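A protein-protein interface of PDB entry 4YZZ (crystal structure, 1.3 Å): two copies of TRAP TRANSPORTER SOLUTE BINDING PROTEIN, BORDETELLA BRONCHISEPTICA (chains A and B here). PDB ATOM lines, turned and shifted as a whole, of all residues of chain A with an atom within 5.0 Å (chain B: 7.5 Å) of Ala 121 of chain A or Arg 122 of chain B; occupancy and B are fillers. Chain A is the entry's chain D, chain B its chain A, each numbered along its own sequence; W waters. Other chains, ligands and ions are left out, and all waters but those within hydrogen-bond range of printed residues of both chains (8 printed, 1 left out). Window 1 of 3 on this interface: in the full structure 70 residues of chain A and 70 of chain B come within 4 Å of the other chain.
Of chain B, only Arg 122 comes within 4 Å of Ala 121 of chain A. Of chain A, only Ala 121, Leu 278 and Asp 282 come within 4 Å of Arg 122 of chain B. Printed residues of chain B within 4 Å of Val 156 of chain A: Trp 345 and Glu 350. Of the printed residues of chain B, Asp 282 of chain A touches Arg 122, Ala 126, Glu 342 and Phe 346. Gly 242 of chain B touches none of the printed residues of chain A. The nearest residue of chain B that does not touch Ala 121 of chain A is Glu 350 of chain B (5.4 Å). The nearest printed residue of chain A that does not touch Ala 279 of chain B is Arg 122 of chain A (5.1 Å).
Arg 122 of chain A touches Leu 278 of chain B, and with the chains exchanged Leu 278 of chain A touches Arg 122 of chain B. 12 positions are printed for both chains. Of the 16 pairs that touch across the chains among the printed residues, 6 have their exchanged pair printed and touching as well.
OE1 of Glu 350 of chain B is in salt-bridge range of NH2 of Arg 122 of chain B, 2.8 Å away. N of Arg 122 of chain A lies within hydrogen-bond range of OD1 of Asn 120 of chain A (3.3 Å). The side-chain amide oxygen of Asn 153 of chain A lies within hydrogen-bond range of the backbone NH of Gly 155 of chain A, 2.9 Å away.
Water W1 lies within hydrogen-bond range of OE2 of Glu 350 of chain B, OG of Ser 243 of chain A, N of Ala 121 of chain A and NH1 of Arg 122 of chain B. Water W7 bridges the side-chain carboxylate (OD1) of Asp 282 of chain A (2.7 Å) and the indole nitrogen (NE1) of Trp 345 of chain B (2.8 Å).
Arg 122 of chain B touches Ala 121 of chain A (NH1 to CB, 3.9 Å). Asn 125 of chain A touches Met 275 of chain B (ND2 to CG, 3.8 Å). CB of Ala 279 of chain B touches O of Asn 125 of chain A, at 3.99 Å. Glu 350 of chain B touches Gly 155 of chain A. Trp 345 of chain B touches Val 156 of chain A (CZ2 to O, 3.9 Å). Asp 282 of chain A touches Ala 126 of chain B.
Printed residues of chain B that touch a printed residue of chain A: Arg 122, Ala 126, Met 275, Leu 278, Ala 279, Asp 282, Glu 342, Trp 345, Phe 346, Glu 350 and Asp 354. Of the 14 printed residues of chain A, 9 touch a printed residue of chain B. Hydrophobic or aromatic side chains of chain A that line the printed part of chain B: Ala 121, Ala 126, Val 156 and Leu 278. Among the printed residues, 16 pairs touch across the chains.
The side-chain carboxylate (OD1) of Asp 282 of chain A lies within salt-bridge range of the guanidinium group (NH2) of Arg 122 of chain B, 2.8 Å away. The side-chain carboxylate of Asp 282 of chain B is in salt-bridge range of the guanidinium group of Arg 122 of chain A, at 2.8 Å. O of Asp 282 of chain A lies close to OE2 of Glu 342 of chain B, 2.6 Å away. The side-chain carboxylate (OE1) of Glu 350 of chain B sits at hydrogen-bond distance from the backbone NH (N) of Val 156 of chain A (2.8 Å). The side-chain amide nitrogen of Asn 120 of chain A sits at hydrogen-bond distance from the side-chain carboxylate of Asp 354 of chain B, 3.0 Å away.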
ATOM      1  N   LEU A 119     -22.262 -26.759  33.391  1.00  0.00           N
ATOM      2  CA  LEU A 119     -21.095 -27.625  33.468  1.00  0.00           C
ATOM      3  C   LEU A 119     -20.013 -27.135  32.512  1.00  0.00           C
ATOM      4  O   LEU A 119     -20.295 -26.554  31.467  1.00  0.00           O
ATOM      5  CB  LEU A 119     -21.521 -29.038  33.081  1.00  0.00           C
ATOM      6  CG  LEU A 119     -22.586 -29.700  33.971  1.00  0.00           C
ATOM      7  CD1 LEU A 119     -22.991 -31.059  33.425  1.00  0.00           C
ATOM      8  CD2 LEU A 119     -22.123 -29.804  35.438  1.00  0.00           C
ATOM      9  N   ASN A 120     -18.753 -27.403  32.824  1.00  0.00           N
ATOM     10  CA  ASN A 120     -17.707 -27.203  31.817  1.00  0.00           C
ATOM     11  C   ASN A 120     -17.729 -28.378  30.825  1.00  0.00           C
ATOM     12  O   ASN A 120     -18.519 -29.315  30.995  1.00  0.00           O
ATOM     13  CB  ASN A 120     -16.314 -26.904  32.430  1.00  0.00           C
ATOM     14  CG  ASN A 120     -15.670 -28.079  33.122  1.00  0.00           C
ATOM     15  OD1 ASN A 120     -16.010 -29.215  32.894  1.00  0.00           O
ATOM     16  ND2 ASN A 120     -14.689 -27.782  33.977  1.00  0.00           N
ATOM     17  N   ALA A 121     -16.929 -28.318  29.763  1.00  0.00           N
ATOM     18  CA  ALA A 121     -17.027 -29.334  28.721  1.00  0.00           C
ATOM     19  C   ALA A 121     -16.752 -30.727  29.271  1.00  0.00           C
ATOM     20  O   ALA A 121     -17.476 -31.692  28.966  1.00  0.00           O
ATOM     21  CB  ALA A 121     -16.077 -29.025  27.571  1.00  0.00           C
ATOM     22  N   ARG A 122     -15.680 -30.872  30.055  1.00  0.00           N
ATOM     23  CA  ARG A 122     -15.390 -32.167  30.668  1.00  0.00           C
ATOM     24  C   ARG A 122     -16.554 -32.663  31.511  1.00  0.00           C
ATOM     25  O   ARG A 122     -16.937 -33.825  31.434  1.00  0.00           O
ATOM     26  CB  ARG A 122     -14.125 -32.122  31.522  1.00  0.00           C
ATOM     27  CG  ARG A 122     -12.894 -32.455  30.690  1.00  0.00           C
ATOM     28  CD  ARG A 122     -11.614 -32.293  31.425  1.00  0.00           C
ATOM     29  NE  ARG A 122     -11.546 -33.036  32.668  1.00  0.00           N
ATOM     30  CZ  ARG A 122     -10.487 -32.975  33.451  1.00  0.00           C
ATOM     31  NH1 ARG A 122      -9.466 -32.210  33.071  1.00  0.00           N
ATOM     32  NH2 ARG A 122     -10.461 -33.625  34.593  1.00  0.00           N
ATOM     33  N   GLN A 123     -17.111 -31.787  32.333  1.00  0.00           N
ATOM     34  CA  GLN A 123     -18.171 -32.206  33.235  1.00  0.00           C
ATOM     35  C   GLN A 123     -19.438 -32.599  32.484  1.00  0.00           C
ATOM     36  O   GLN A 123     -20.159 -33.510  32.887  1.00  0.00           O
ATOM     37  CB  GLN A 123     -18.451 -31.091  34.227  1.00  0.00           C
ATOM     38  CG  GLN A 123     -17.273 -30.856  35.178  1.00  0.00           C
ATOM     39  CD  GLN A 123     -17.378 -29.533  35.912  1.00  0.00           C
ATOM     40  OE1 GLN A 123     -18.232 -28.689  35.588  1.00  0.00           O
ATOM     41  NE2 GLN A 123     -16.517 -29.341  36.895  1.00  0.00           N
ATOM     42  N   HIS A 124     -19.712 -31.900  31.390  1.00  0.00           N
ATOM     43  CA  HIS A 124     -20.868 -32.222  30.557  1.00  0.00           C
ATOM     44  C   HIS A 124     -20.701 -33.585  29.898  1.00  0.00           C
ATOM     45  O   HIS A 124     -21.594 -34.425  29.955  1.00  0.00           O
ATOM     46  CB  HIS A 124     -21.081 -31.157  29.503  1.00  0.00           C
ATOM     47  CG  HIS A 124     -22.276 -31.397  28.640  1.00  0.00           C
ATOM     48  ND1 HIS A 124     -23.568 -31.177  29.076  1.00  0.00           N
ATOM     49  CD2 HIS A 124     -22.370 -31.838  27.364  1.00  0.00           C
ATOM     50  CE1 HIS A 124     -24.406 -31.467  28.093  1.00  0.00           C
ATOM     51  NE2 HIS A 124     -23.705 -31.841  27.035  1.00  0.00           N
ATOM     52  N   ASN A 125     -19.531 -33.844  29.319  1.00  0.00           N
ATOM     53  CA  ASN A 125     -19.309 -35.164  28.752  1.00  0.00           C
ATOM     54  C   ASN A 125     -19.352 -36.274  29.812  1.00  0.00           C
ATOM     55  O   ASN A 125     -19.826 -37.387  29.539  1.00  0.00           O
ATOM     56  CB  ASN A 125     -18.027 -35.191  27.932  1.00  0.00           C
ATOM     57  CG  ASN A 125     -18.159 -34.402  26.645  1.00  0.00           C
ATOM     58  OD1 ASN A 125     -19.266 -34.210  26.131  1.00  0.00           O
ATOM     59  ND2 ASN A 125     -17.039 -33.929  26.123  1.00  0.00           N
ATOM     60  N   ALA A 126     -18.884 -35.966  31.022  1.00  0.00           N
ATOM     61  CA  ALA A 126     -18.974 -36.925  32.124  1.00  0.00           C
ATOM     62  C   ALA A 126     -20.432 -37.197  32.497  1.00  0.00           C
ATOM     63  O   ALA A 126     -20.845 -38.355  32.678  1.00  0.00           O
ATOM     64  CB  ALA A 126     -18.200 -36.406  33.338  1.00  0.00           C
ATOM     65  N   ASN A 153     -18.115 -29.695  21.163  1.00  0.00           N
ATOM     66  CA  ASN A 153     -18.265 -28.664  22.181  1.00  0.00           C
ATOM     67  C   ASN A 153     -17.476 -27.464  21.692  1.00  0.00           C
ATOM     68  O   ASN A 153     -16.401 -27.612  21.098  1.00  0.00           O
ATOM     69  CB  ASN A 153     -17.791 -29.150  23.564  1.00  0.00           C
ATOM     70  CG  ASN A 153     -18.365 -28.309  24.704  1.00  0.00           C
ATOM     71  OD1 ASN A 153     -17.946 -27.165  24.936  1.00  0.00           O
ATOM     72  ND2 ASN A 153     -19.306 -28.887  25.444  1.00  0.00           N
ATOM     73  N   GLY A 155     -16.524 -24.980  23.724  1.00  0.00           N
ATOM     74  CA  GLY A 155     -15.792 -24.403  24.840  1.00  0.00           C
ATOM     75  C   GLY A 155     -16.450 -23.119  25.299  1.00  0.00           C
ATOM     76  O   GLY A 155     -17.402 -22.627  24.676  1.00  0.00           O
ATOM     77  N   VAL A 156     -15.971 -22.562  26.396  1.00  0.00           N
ATOM     78  CA  VAL A 156     -16.458 -21.276  26.871  1.00  0.00           C
ATOM     79  C   VAL A 156     -16.163 -20.222  25.817  1.00  0.00           C
ATOM     80  O   VAL A 156     -15.094 -20.173  25.219  1.00  0.00           O
ATOM     81  CB  VAL A 156     -15.845 -20.920  28.263  1.00  0.00           C
ATOM     82  CG1 VAL A 156     -16.190 -19.495  28.688  1.00  0.00           C
ATOM     83  CG2 VAL A 156     -16.341 -21.922  29.304  1.00  0.00           C
ATOM     84  N   SER A 243     -20.732 -24.225  28.433  1.00  0.00           N
ATOM     85  CA  SER A 243     -19.758 -24.703  27.457  1.00  0.00           C
ATOM     86  C   SER A 243     -20.549 -25.490  26.423  1.00  0.00           C
ATOM     87  O   SER A 243     -20.807 -26.678  26.605  1.00  0.00           O
ATOM     88  CB  SER A 243     -18.684 -25.578  28.114  1.00  0.00           C
ATOM     89  OG  SER A 243     -17.597 -25.806  27.233  1.00  0.00           O
ATOM     90  N   LEU A 278     -13.547 -29.484  20.057  1.00  0.00           N
ATOM     91  CA  LEU A 278     -13.072 -28.664  21.148  1.00  0.00           C
ATOM     92  C   LEU A 278     -11.559 -28.486  21.115  1.00  0.00           C
ATOM     93  O   LEU A 278     -11.055 -27.392  21.377  1.00  0.00           O
ATOM     94  CB  LEU A 278     -13.540 -29.277  22.460  1.00  0.00           C
ATOM     95  CG  LEU A 278     -13.193 -28.523  23.735  1.00  0.00           C
ATOM     96  CD1 LEU A 278     -13.817 -27.169  23.716  1.00  0.00           C
ATOM     97  CD2 LEU A 278     -13.669 -29.311  24.938  1.00  0.00           C
ATOM     98  N   ASP A 282      -9.651 -24.985  20.985  1.00  0.00           N
ATOM     99  CA  ASP A 282      -8.633 -24.676  21.983  1.00  0.00           C
ATOM    100  C   ASP A 282      -7.311 -24.282  21.321  1.00  0.00           C
ATOM    101  O   ASP A 282      -6.624 -23.363  21.795  1.00  0.00           O
ATOM    102  CB  ASP A 282      -8.407 -25.859  22.922  1.00  0.00           C
ATOM    103  CG  ASP A 282      -9.529 -26.057  23.954  1.00  0.00           C
ATOM    104  OD1 ASP A 282     -10.376 -25.158  24.140  1.00  0.00           O
ATOM    105  OD2 ASP A 282      -9.568 -27.139  24.586  1.00  0.00           O
ATOM    106  N   LEU B 119       0.727 -28.897  30.095  1.00  0.00           N
ATOM    107  CA  LEU B 119      -0.596 -28.678  29.533  1.00  0.00           C
ATOM    108  C   LEU B 119      -1.658 -29.444  30.324  1.00  0.00           C
ATOM    109  O   LEU B 119      -1.428 -30.567  30.761  1.00  0.00           O
ATOM    110  CB  LEU B 119      -0.604 -29.181  28.089  1.00  0.00           C
ATOM    111  CG  LEU B 119       0.397 -28.528  27.121  1.00  0.00           C
ATOM    112  CD1 LEU B 119       0.296 -29.179  25.752  1.00  0.00           C
ATOM    113  CD2 LEU B 119       0.182 -27.036  27.022  1.00  0.00           C
ATOM    114  N   ASN B 120      -2.852 -28.865  30.475  1.00  0.00           N
ATOM    115  CA  ASN B 120      -3.942 -29.650  31.029  1.00  0.00           C
ATOM    116  C   ASN B 120      -4.492 -30.591  29.950  1.00  0.00           C
ATOM    117  O   ASN B 120      -4.039 -30.561  28.808  1.00  0.00           O
ATOM    118  CB  ASN B 120      -5.025 -28.776  31.698  1.00  0.00           C
ATOM    119  CG  ASN B 120      -5.819 -27.931  30.734  1.00  0.00           C
ATOM    120  OD1 ASN B 120      -5.895 -28.227  29.546  1.00  0.00           O
ATOM    121  ND2 ASN B 120      -6.439 -26.875  31.251  1.00  0.00           N
ATOM    122  N   ALA B 121      -5.433 -31.456  30.311  1.00  0.00           N
ATOM    123  CA  ALA B 121      -5.876 -32.489  29.396  1.00  0.00           C
ATOM    124  C   ALA B 121      -6.391 -31.905  28.072  1.00  0.00           C
ATOM    125  O   ALA B 121      -6.047 -32.378  26.983  1.00  0.00           O
ATOM    126  CB  ALA B 121      -6.948 -33.354  30.062  1.00  0.00           C
ATOM    127  N   ARG B 122      -7.254 -30.901  28.155  1.00  0.00           N
ATOM    128  CA  ARG B 122      -7.757 -30.257  26.948  1.00  0.00           C
ATOM    129  C   ARG B 122      -6.652 -29.674  26.111  1.00  0.00           C
ATOM    130  O   ARG B 122      -6.605 -29.864  24.894  1.00  0.00           O
ATOM    131  CB  ARG B 122      -8.743 -29.161  27.301  1.00  0.00           C
ATOM    132  CG  ARG B 122     -10.128 -29.781  27.354  1.00  0.00           C
ATOM    133  CD  ARG B 122     -11.205 -28.832  27.706  1.00  0.00           C
ATOM    134  NE  ARG B 122     -11.230 -27.637  26.866  1.00  0.00           N
ATOM    135  CZ  ARG B 122     -12.071 -26.650  27.091  1.00  0.00           C
ATOM    136  NH1 ARG B 122     -12.899 -26.748  28.121  1.00  0.00           N
ATOM    137  NH2 ARG B 122     -12.057 -25.571  26.343  1.00  0.00           N
ATOM    138  N   GLN B 123      -5.752 -28.956  26.754  1.00  0.00           N
ATOM    139  CA  GLN B 123      -4.662 -28.320  26.038  1.00  0.00           C
ATOM    140  C   GLN B 123      -3.723 -29.349  25.401  1.00  0.00           C
ATOM    141  O   GLN B 123      -3.170 -29.130  24.318  1.00  0.00           O
ATOM    142  CB  GLN B 123      -3.895 -27.405  26.978  1.00  0.00           C
ATOM    143  CG  GLN B 123      -4.711 -26.238  27.501  1.00  0.00           C
ATOM    144  CD  GLN B 123      -4.045 -25.530  28.665  1.00  0.00           C
ATOM    145  OE1 GLN B 123      -3.077 -26.043  29.250  1.00  0.00           O
ATOM    146  NE2 GLN B 123      -4.566 -24.374  29.036  1.00  0.00           N
ATOM    147  N   HIS B 124      -3.551 -30.476  26.078  1.00  0.00           N
ATOM    148  CA  HIS B 124      -2.702 -31.533  25.568  1.00  0.00           C
ATOM    149  C   HIS B 124      -3.323 -32.136  24.307  1.00  0.00           C
ATOM    150  O   HIS B 124      -2.645 -32.289  23.294  1.00  0.00           O
ATOM    151  CB  HIS B 124      -2.506 -32.593  26.637  1.00  0.00           C
ATOM    152  CG  HIS B 124      -1.634 -33.726  26.200  1.00  0.00           C
ATOM    153  ND1 HIS B 124      -0.267 -33.610  26.025  1.00  0.00           N
ATOM    154  CD2 HIS B 124      -1.950 -35.001  25.882  1.00  0.00           C
ATOM    155  CE1 HIS B 124       0.216 -34.774  25.625  1.00  0.00           C
ATOM    156  NE2 HIS B 124      -0.781 -35.637  25.551  1.00  0.00           N
ATOM    157  N   ASN B 125      -4.623 -32.439  24.335  1.00  0.00           N
ATOM    158  CA  ASN B 125      -5.245 -33.004  23.146  1.00  0.00           C
ATOM    159  C   ASN B 125      -5.260 -31.970  22.010  1.00  0.00           C
ATOM    160  O   ASN B 125      -5.122 -32.327  20.817  1.00  0.00           O
ATOM    161  CB  ASN B 125      -6.646 -33.534  23.460  1.00  0.00           C
ATOM    162  CG  ASN B 125      -6.611 -34.837  24.237  1.00  0.00           C
ATOM    163  OD1 ASN B 125      -5.646 -35.578  24.155  1.00  0.00           O
ATOM    164  ND2 ASN B 125      -7.644 -35.102  25.018  1.00  0.00           N
ATOM    165  N   ALA B 126      -5.411 -30.697  22.352  1.00  0.00           N
ATOM    166  CA  ALA B 126      -5.299 -29.636  21.355  1.00  0.00           C
ATOM    167  C   ALA B 126      -3.909 -29.618  20.717  1.00  0.00           C
ATOM    168  O   ALA B 126      -3.765 -29.572  19.497  1.00  0.00           O
ATOM    169  CB  ALA B 126      -5.619 -28.283  21.972  1.00  0.00           C
ATOM    170  N   TRP B 127      -2.863 -29.697  21.537  1.00  0.00           N
ATOM    171  CA  TRP B 127      -1.491 -29.702  21.005  1.00  0.00           C
ATOM    172  C   TRP B 127      -1.264 -30.923  20.099  1.00  0.00           C
ATOM    173  O   TRP B 127      -0.740 -30.818  18.991  1.00  0.00           O
ATOM    174  CB  TRP B 127      -0.459 -29.712  22.140  1.00  0.00           C
ATOM    175  CG  TRP B 127       0.942 -29.672  21.622  1.00  0.00           C
ATOM    176  CD1 TRP B 127       1.526 -28.668  20.921  1.00  0.00           C
ATOM    177  CD2 TRP B 127       1.940 -30.688  21.770  1.00  0.00           C
ATOM    178  NE1 TRP B 127       2.819 -28.992  20.602  1.00  0.00           N
ATOM    179  CE2 TRP B 127       3.098 -30.226  21.115  1.00  0.00           C
ATOM    180  CE3 TRP B 127       1.960 -31.945  22.382  1.00  0.00           C
ATOM    181  CZ2 TRP B 127       4.271 -30.966  21.064  1.00  0.00           C
ATOM    182  CZ3 TRP B 127       3.137 -32.681  22.341  1.00  0.00           C
ATOM    183  CH2 TRP B 127       4.272 -32.188  21.675  1.00  0.00           C
ATOM    184  N   ILE B 128      -1.677 -32.081  20.589  1.00  0.00           N
ATOM    185  CA  ILE B 128      -1.503 -33.334  19.855  1.00  0.00           C
ATOM    186  C   ILE B 128      -2.162 -33.282  18.485  1.00  0.00           C
ATOM    187  O   ILE B 128      -1.535 -33.571  17.463  1.00  0.00           O
ATOM    188  CB  ILE B 128      -2.051 -34.512  20.681  1.00  0.00           C
ATOM    189  CG1 ILE B 128      -1.182 -34.729  21.939  1.00  0.00           C
ATOM    190  CG2 ILE B 128      -2.152 -35.793  19.820  1.00  0.00           C
ATOM    191  CD1 ILE B 128       0.196 -35.359  21.718  1.00  0.00           C
ATOM    192  N   ASN B 153      -6.806 -40.042  29.210  1.00  0.00           N
ATOM    193  CA  ASN B 153      -6.208 -39.075  30.101  1.00  0.00           C
ATOM    194  C   ASN B 153      -6.876 -39.249  31.446  1.00  0.00           C
ATOM    195  O   ASN B 153      -8.060 -39.582  31.520  1.00  0.00           O
ATOM    196  CB  ASN B 153      -6.465 -37.665  29.570  1.00  0.00           C
ATOM    197  CG  ASN B 153      -5.471 -36.642  30.091  1.00  0.00           C
ATOM    198  OD1 ASN B 153      -5.453 -36.332  31.289  1.00  0.00           O
ATOM    199  ND2 ASN B 153      -4.662 -36.086  29.206  1.00  0.00           N
ATOM    200  N   GLY B 242       0.852 -31.900  33.943  1.00  0.00           N
ATOM    201  CA  GLY B 242      -0.326 -31.070  33.773  1.00  0.00           C
ATOM    202  C   GLY B 242      -1.587 -31.897  33.590  1.00  0.00           C
ATOM    203  O   GLY B 242      -2.692 -31.476  33.949  1.00  0.00           O
ATOM    204  N   SER B 243      -1.417 -33.053  32.962  1.00  0.00           N
ATOM    205  CA  SER B 243      -2.434 -34.069  32.793  1.00  0.00           C
ATOM    206  C   SER B 243      -1.631 -35.327  32.490  1.00  0.00           C
ATOM    207  O   SER B 243      -0.617 -35.250  31.806  1.00  0.00           O
ATOM    208  CB  SER B 243      -3.402 -33.720  31.653  1.00  0.00           C
ATOM    209  OG  SER B 243      -2.924 -34.120  30.365  1.00  0.00           O
ATOM    210  N   MET B 275     -11.746 -38.942  25.130  1.00  0.00           N
ATOM    211  CA  MET B 275     -12.829 -38.284  25.858  1.00  0.00           C
ATOM    212  C   MET B 275     -13.396 -39.176  26.962  1.00  0.00           C
ATOM    213  O   MET B 275     -13.600 -38.725  28.079  1.00  0.00           O
ATOM    214  CB  MET B 275     -13.937 -37.860  24.882  1.00  0.00           C
ATOM    215  CG  MET B 275     -15.152 -37.227  25.542  1.00  0.00           C
ATOM    216  SD  MET B 275     -16.392 -38.399  26.088  1.00  0.00           S
ATOM    217  CE  MET B 275     -17.022 -38.999  24.506  1.00  0.00           C
ATOM    218  N   LEU B 278     -11.460 -40.037  30.566  1.00  0.00           N
ATOM    219  CA  LEU B 278     -11.474 -38.887  31.453  1.00  0.00           C
ATOM    220  C   LEU B 278     -12.882 -38.577  31.938  1.00  0.00           C
ATOM    221  O   LEU B 278     -13.076 -38.166  33.096  1.00  0.00           O
ATOM    222  CB  LEU B 278     -10.857 -37.687  30.752  1.00  0.00           C
ATOM    223  CG  LEU B 278     -10.676 -36.438  31.599  1.00  0.00           C
ATOM    224  CD1 LEU B 278      -9.894 -36.745  32.885  1.00  0.00           C
ATOM    225  CD2 LEU B 278      -9.960 -35.390  30.746  1.00  0.00           C
ATOM    226  N   ALA B 279     -13.877 -38.780  31.090  1.00  0.00           N
ATOM    227  CA  ALA B 279     -15.252 -38.614  31.526  1.00  0.00           C
ATOM    228  C   ALA B 279     -15.622 -39.576  32.658  1.00  0.00           C
ATOM    229  O   ALA B 279     -16.352 -39.221  33.586  1.00  0.00           O
ATOM    230  CB  ALA B 279     -16.185 -38.794  30.344  1.00  0.00           C
ATOM    231  N   ASP B 282     -13.860 -38.259  35.782  1.00  0.00           N
ATOM    232  CA  ASP B 282     -14.561 -37.066  36.237  1.00  0.00           C
ATOM    233  C   ASP B 282     -15.878 -37.438  36.930  1.00  0.00           C
ATOM    234  O   ASP B 282     -16.229 -36.827  37.933  1.00  0.00           O
ATOM    235  CB  ASP B 282     -14.821 -36.118  35.068  1.00  0.00           C
ATOM    236  CG  ASP B 282     -13.579 -35.343  34.644  1.00  0.00           C
ATOM    237  OD1 ASP B 282     -12.559 -35.319  35.386  1.00  0.00           O
ATOM    238  OD2 ASP B 282     -13.612 -34.737  33.538  1.00  0.00           O
ATOM    239  N   PHE B 338       3.159 -23.043  22.680  1.00  0.00           N
ATOM    240  CA  PHE B 338       1.781 -23.512  22.708  1.00  0.00           C
ATOM    241  C   PHE B 338       1.221 -23.404  24.125  1.00  0.00           C
ATOM    242  O   PHE B 338       0.107 -22.935  24.305  1.00  0.00           O
ATOM    243  CB  PHE B 338       1.685 -24.945  22.174  1.00  0.00           C
ATOM    244  CG  PHE B 338       0.275 -25.374  21.827  1.00  0.00           C
ATOM    245  CD1 PHE B 338      -0.288 -25.024  20.614  1.00  0.00           C
ATOM    246  CD2 PHE B 338      -0.486 -26.125  22.705  1.00  0.00           C
ATOM    247  CE1 PHE B 338      -1.575 -25.403  20.274  1.00  0.00           C
ATOM    248  CE2 PHE B 338      -1.778 -26.517  22.363  1.00  0.00           C
ATOM    249  CZ  PHE B 338      -2.319 -26.152  21.158  1.00  0.00           C
ATOM    250  N   GLU B 342      -2.002 -21.231  25.168  1.00  0.00           N
ATOM    251  CA  GLU B 342      -3.116 -21.926  25.796  1.00  0.00           C
ATOM    252  C   GLU B 342      -3.423 -21.383  27.188  1.00  0.00           C
ATOM    253  O   GLU B 342      -4.576 -21.114  27.507  1.00  0.00           O
ATOM    254  CB  GLU B 342      -2.835 -23.434  25.907  1.00  0.00           C
ATOM    255  CG  GLU B 342      -2.769 -24.149  24.578  1.00  0.00           C
ATOM    256  CD  GLU B 342      -4.103 -24.197  23.863  1.00  0.00           C
ATOM    257  OE1 GLU B 342      -4.986 -24.965  24.299  1.00  0.00           O
ATOM    258  OE2 GLU B 342      -4.229 -23.517  22.820  1.00  0.00           O
ATOM    259  N   TRP B 345      -5.169 -17.943  27.225  1.00  0.00           N
ATOM    260  CA  TRP B 345      -6.554 -17.996  26.791  1.00  0.00           C
ATOM    261  C   TRP B 345      -7.440 -18.669  27.839  1.00  0.00           C
ATOM    262  O   TRP B 345      -8.520 -18.176  28.131  1.00  0.00           O
ATOM    263  CB  TRP B 345      -6.634 -18.722  25.436  1.00  0.00           C
ATOM    264  CG  TRP B 345      -8.011 -19.201  25.041  1.00  0.00           C
ATOM    265  CD1 TRP B 345      -8.351 -20.469  24.681  1.00  0.00           C
ATOM    266  CD2 TRP B 345      -9.214 -18.421  24.964  1.00  0.00           C
ATOM    267  NE1 TRP B 345      -9.692 -20.530  24.390  1.00  0.00           N
ATOM    268  CE2 TRP B 345     -10.246 -19.289  24.564  1.00  0.00           C
ATOM    269  CE3 TRP B 345      -9.521 -17.082  25.225  1.00  0.00           C
ATOM    270  CZ2 TRP B 345     -11.563 -18.861  24.397  1.00  0.00           C
ATOM    271  CZ3 TRP B 345     -10.829 -16.659  25.057  1.00  0.00           C
ATOM    272  CH2 TRP B 345     -11.832 -17.547  24.666  1.00  0.00           C
ATOM    273  N   PHE B 346      -6.996 -19.786  28.402  1.00  0.00           N
ATOM    274  CA  PHE B 346      -7.790 -20.448  29.428  1.00  0.00           C
ATOM    275  C   PHE B 346      -7.939 -19.589  30.666  1.00  0.00           C
ATOM    276  O   PHE B 346      -8.967 -19.639  31.331  1.00  0.00           O
ATOM    277  CB  PHE B 346      -7.190 -21.810  29.790  1.00  0.00           C
ATOM    278  CG  PHE B 346      -7.584 -22.933  28.835  1.00  0.00           C
ATOM    279  CD1 PHE B 346      -7.269 -22.884  27.479  1.00  0.00           C
ATOM    280  CD2 PHE B 346      -8.265 -24.050  29.314  1.00  0.00           C
ATOM    281  CE1 PHE B 346      -7.636 -23.921  26.632  1.00  0.00           C
ATOM    282  CE2 PHE B 346      -8.625 -25.079  28.477  1.00  0.00           C
ATOM    283  CZ  PHE B 346      -8.313 -25.021  27.137  1.00  0.00           C
ATOM    284  N   GLU B 350     -12.114 -19.962  30.132  1.00  0.00           N
ATOM    285  CA  GLU B 350     -12.460 -21.205  30.824  1.00  0.00           C
ATOM    286  C   GLU B 350     -12.322 -21.077  32.329  1.00  0.00           C
ATOM    287  O   GLU B 350     -13.223 -21.424  33.087  1.00  0.00           O
ATOM    288  CB  GLU B 350     -11.555 -22.365  30.387  1.00  0.00           C
ATOM    289  CG  GLU B 350     -11.825 -22.905  28.991  1.00  0.00           C
ATOM    290  CD  GLU B 350     -13.220 -23.502  28.799  1.00  0.00           C
ATOM    291  OE1 GLU B 350     -13.631 -23.613  27.619  1.00  0.00           O
ATOM    292  OE2 GLU B 350     -13.899 -23.889  29.782  1.00  0.00           O
ATOM    293  N   ASP B 354     -15.007 -21.104  35.289  1.00  0.00           N
ATOM    294  CA  ASP B 354     -14.992 -22.206  36.253  1.00  0.00           C
ATOM    295  C   ASP B 354     -14.716 -21.721  37.681  1.00  0.00           C
ATOM    296  O   ASP B 354     -15.382 -22.163  38.614  1.00  0.00           O
ATOM    297  CB  ASP B 354     -13.970 -23.305  35.882  1.00  0.00           C
ATOM    298  CG  ASP B 354     -14.423 -24.201  34.727  1.00  0.00           C
ATOM    299  OD1 ASP B 354     -15.585 -24.094  34.310  1.00  0.00           O
ATOM    300  OD2 ASP B 354     -13.591 -25.020  34.273  1.00  0.00           O
HETATM  301  O   HOH W   1     -15.545 -25.822  29.044  1.00  0.00           O
HETATM  302  O   HOH W   2      -9.142 -29.685  23.795  1.00  0.00           O
HETATM  303  O   HOH W   3     -13.165 -25.737  31.677  1.00  0.00           O
HETATM  304  O   HOH W   4     -12.762 -21.641  25.891  1.00  0.00           O
HETATM  305  O   HOH W   5     -14.697 -35.527  31.198  1.00  0.00           O
HETATM  306  O   HOH W   6     -11.688 -26.837  35.421  1.00  0.00           O
HETATM  307  O   HOH W   7     -11.302 -22.697  23.477  1.00  0.00           O
HETATM  308  O   HOH W   8      -8.630 -30.175  30.940  1.00  0.00           O
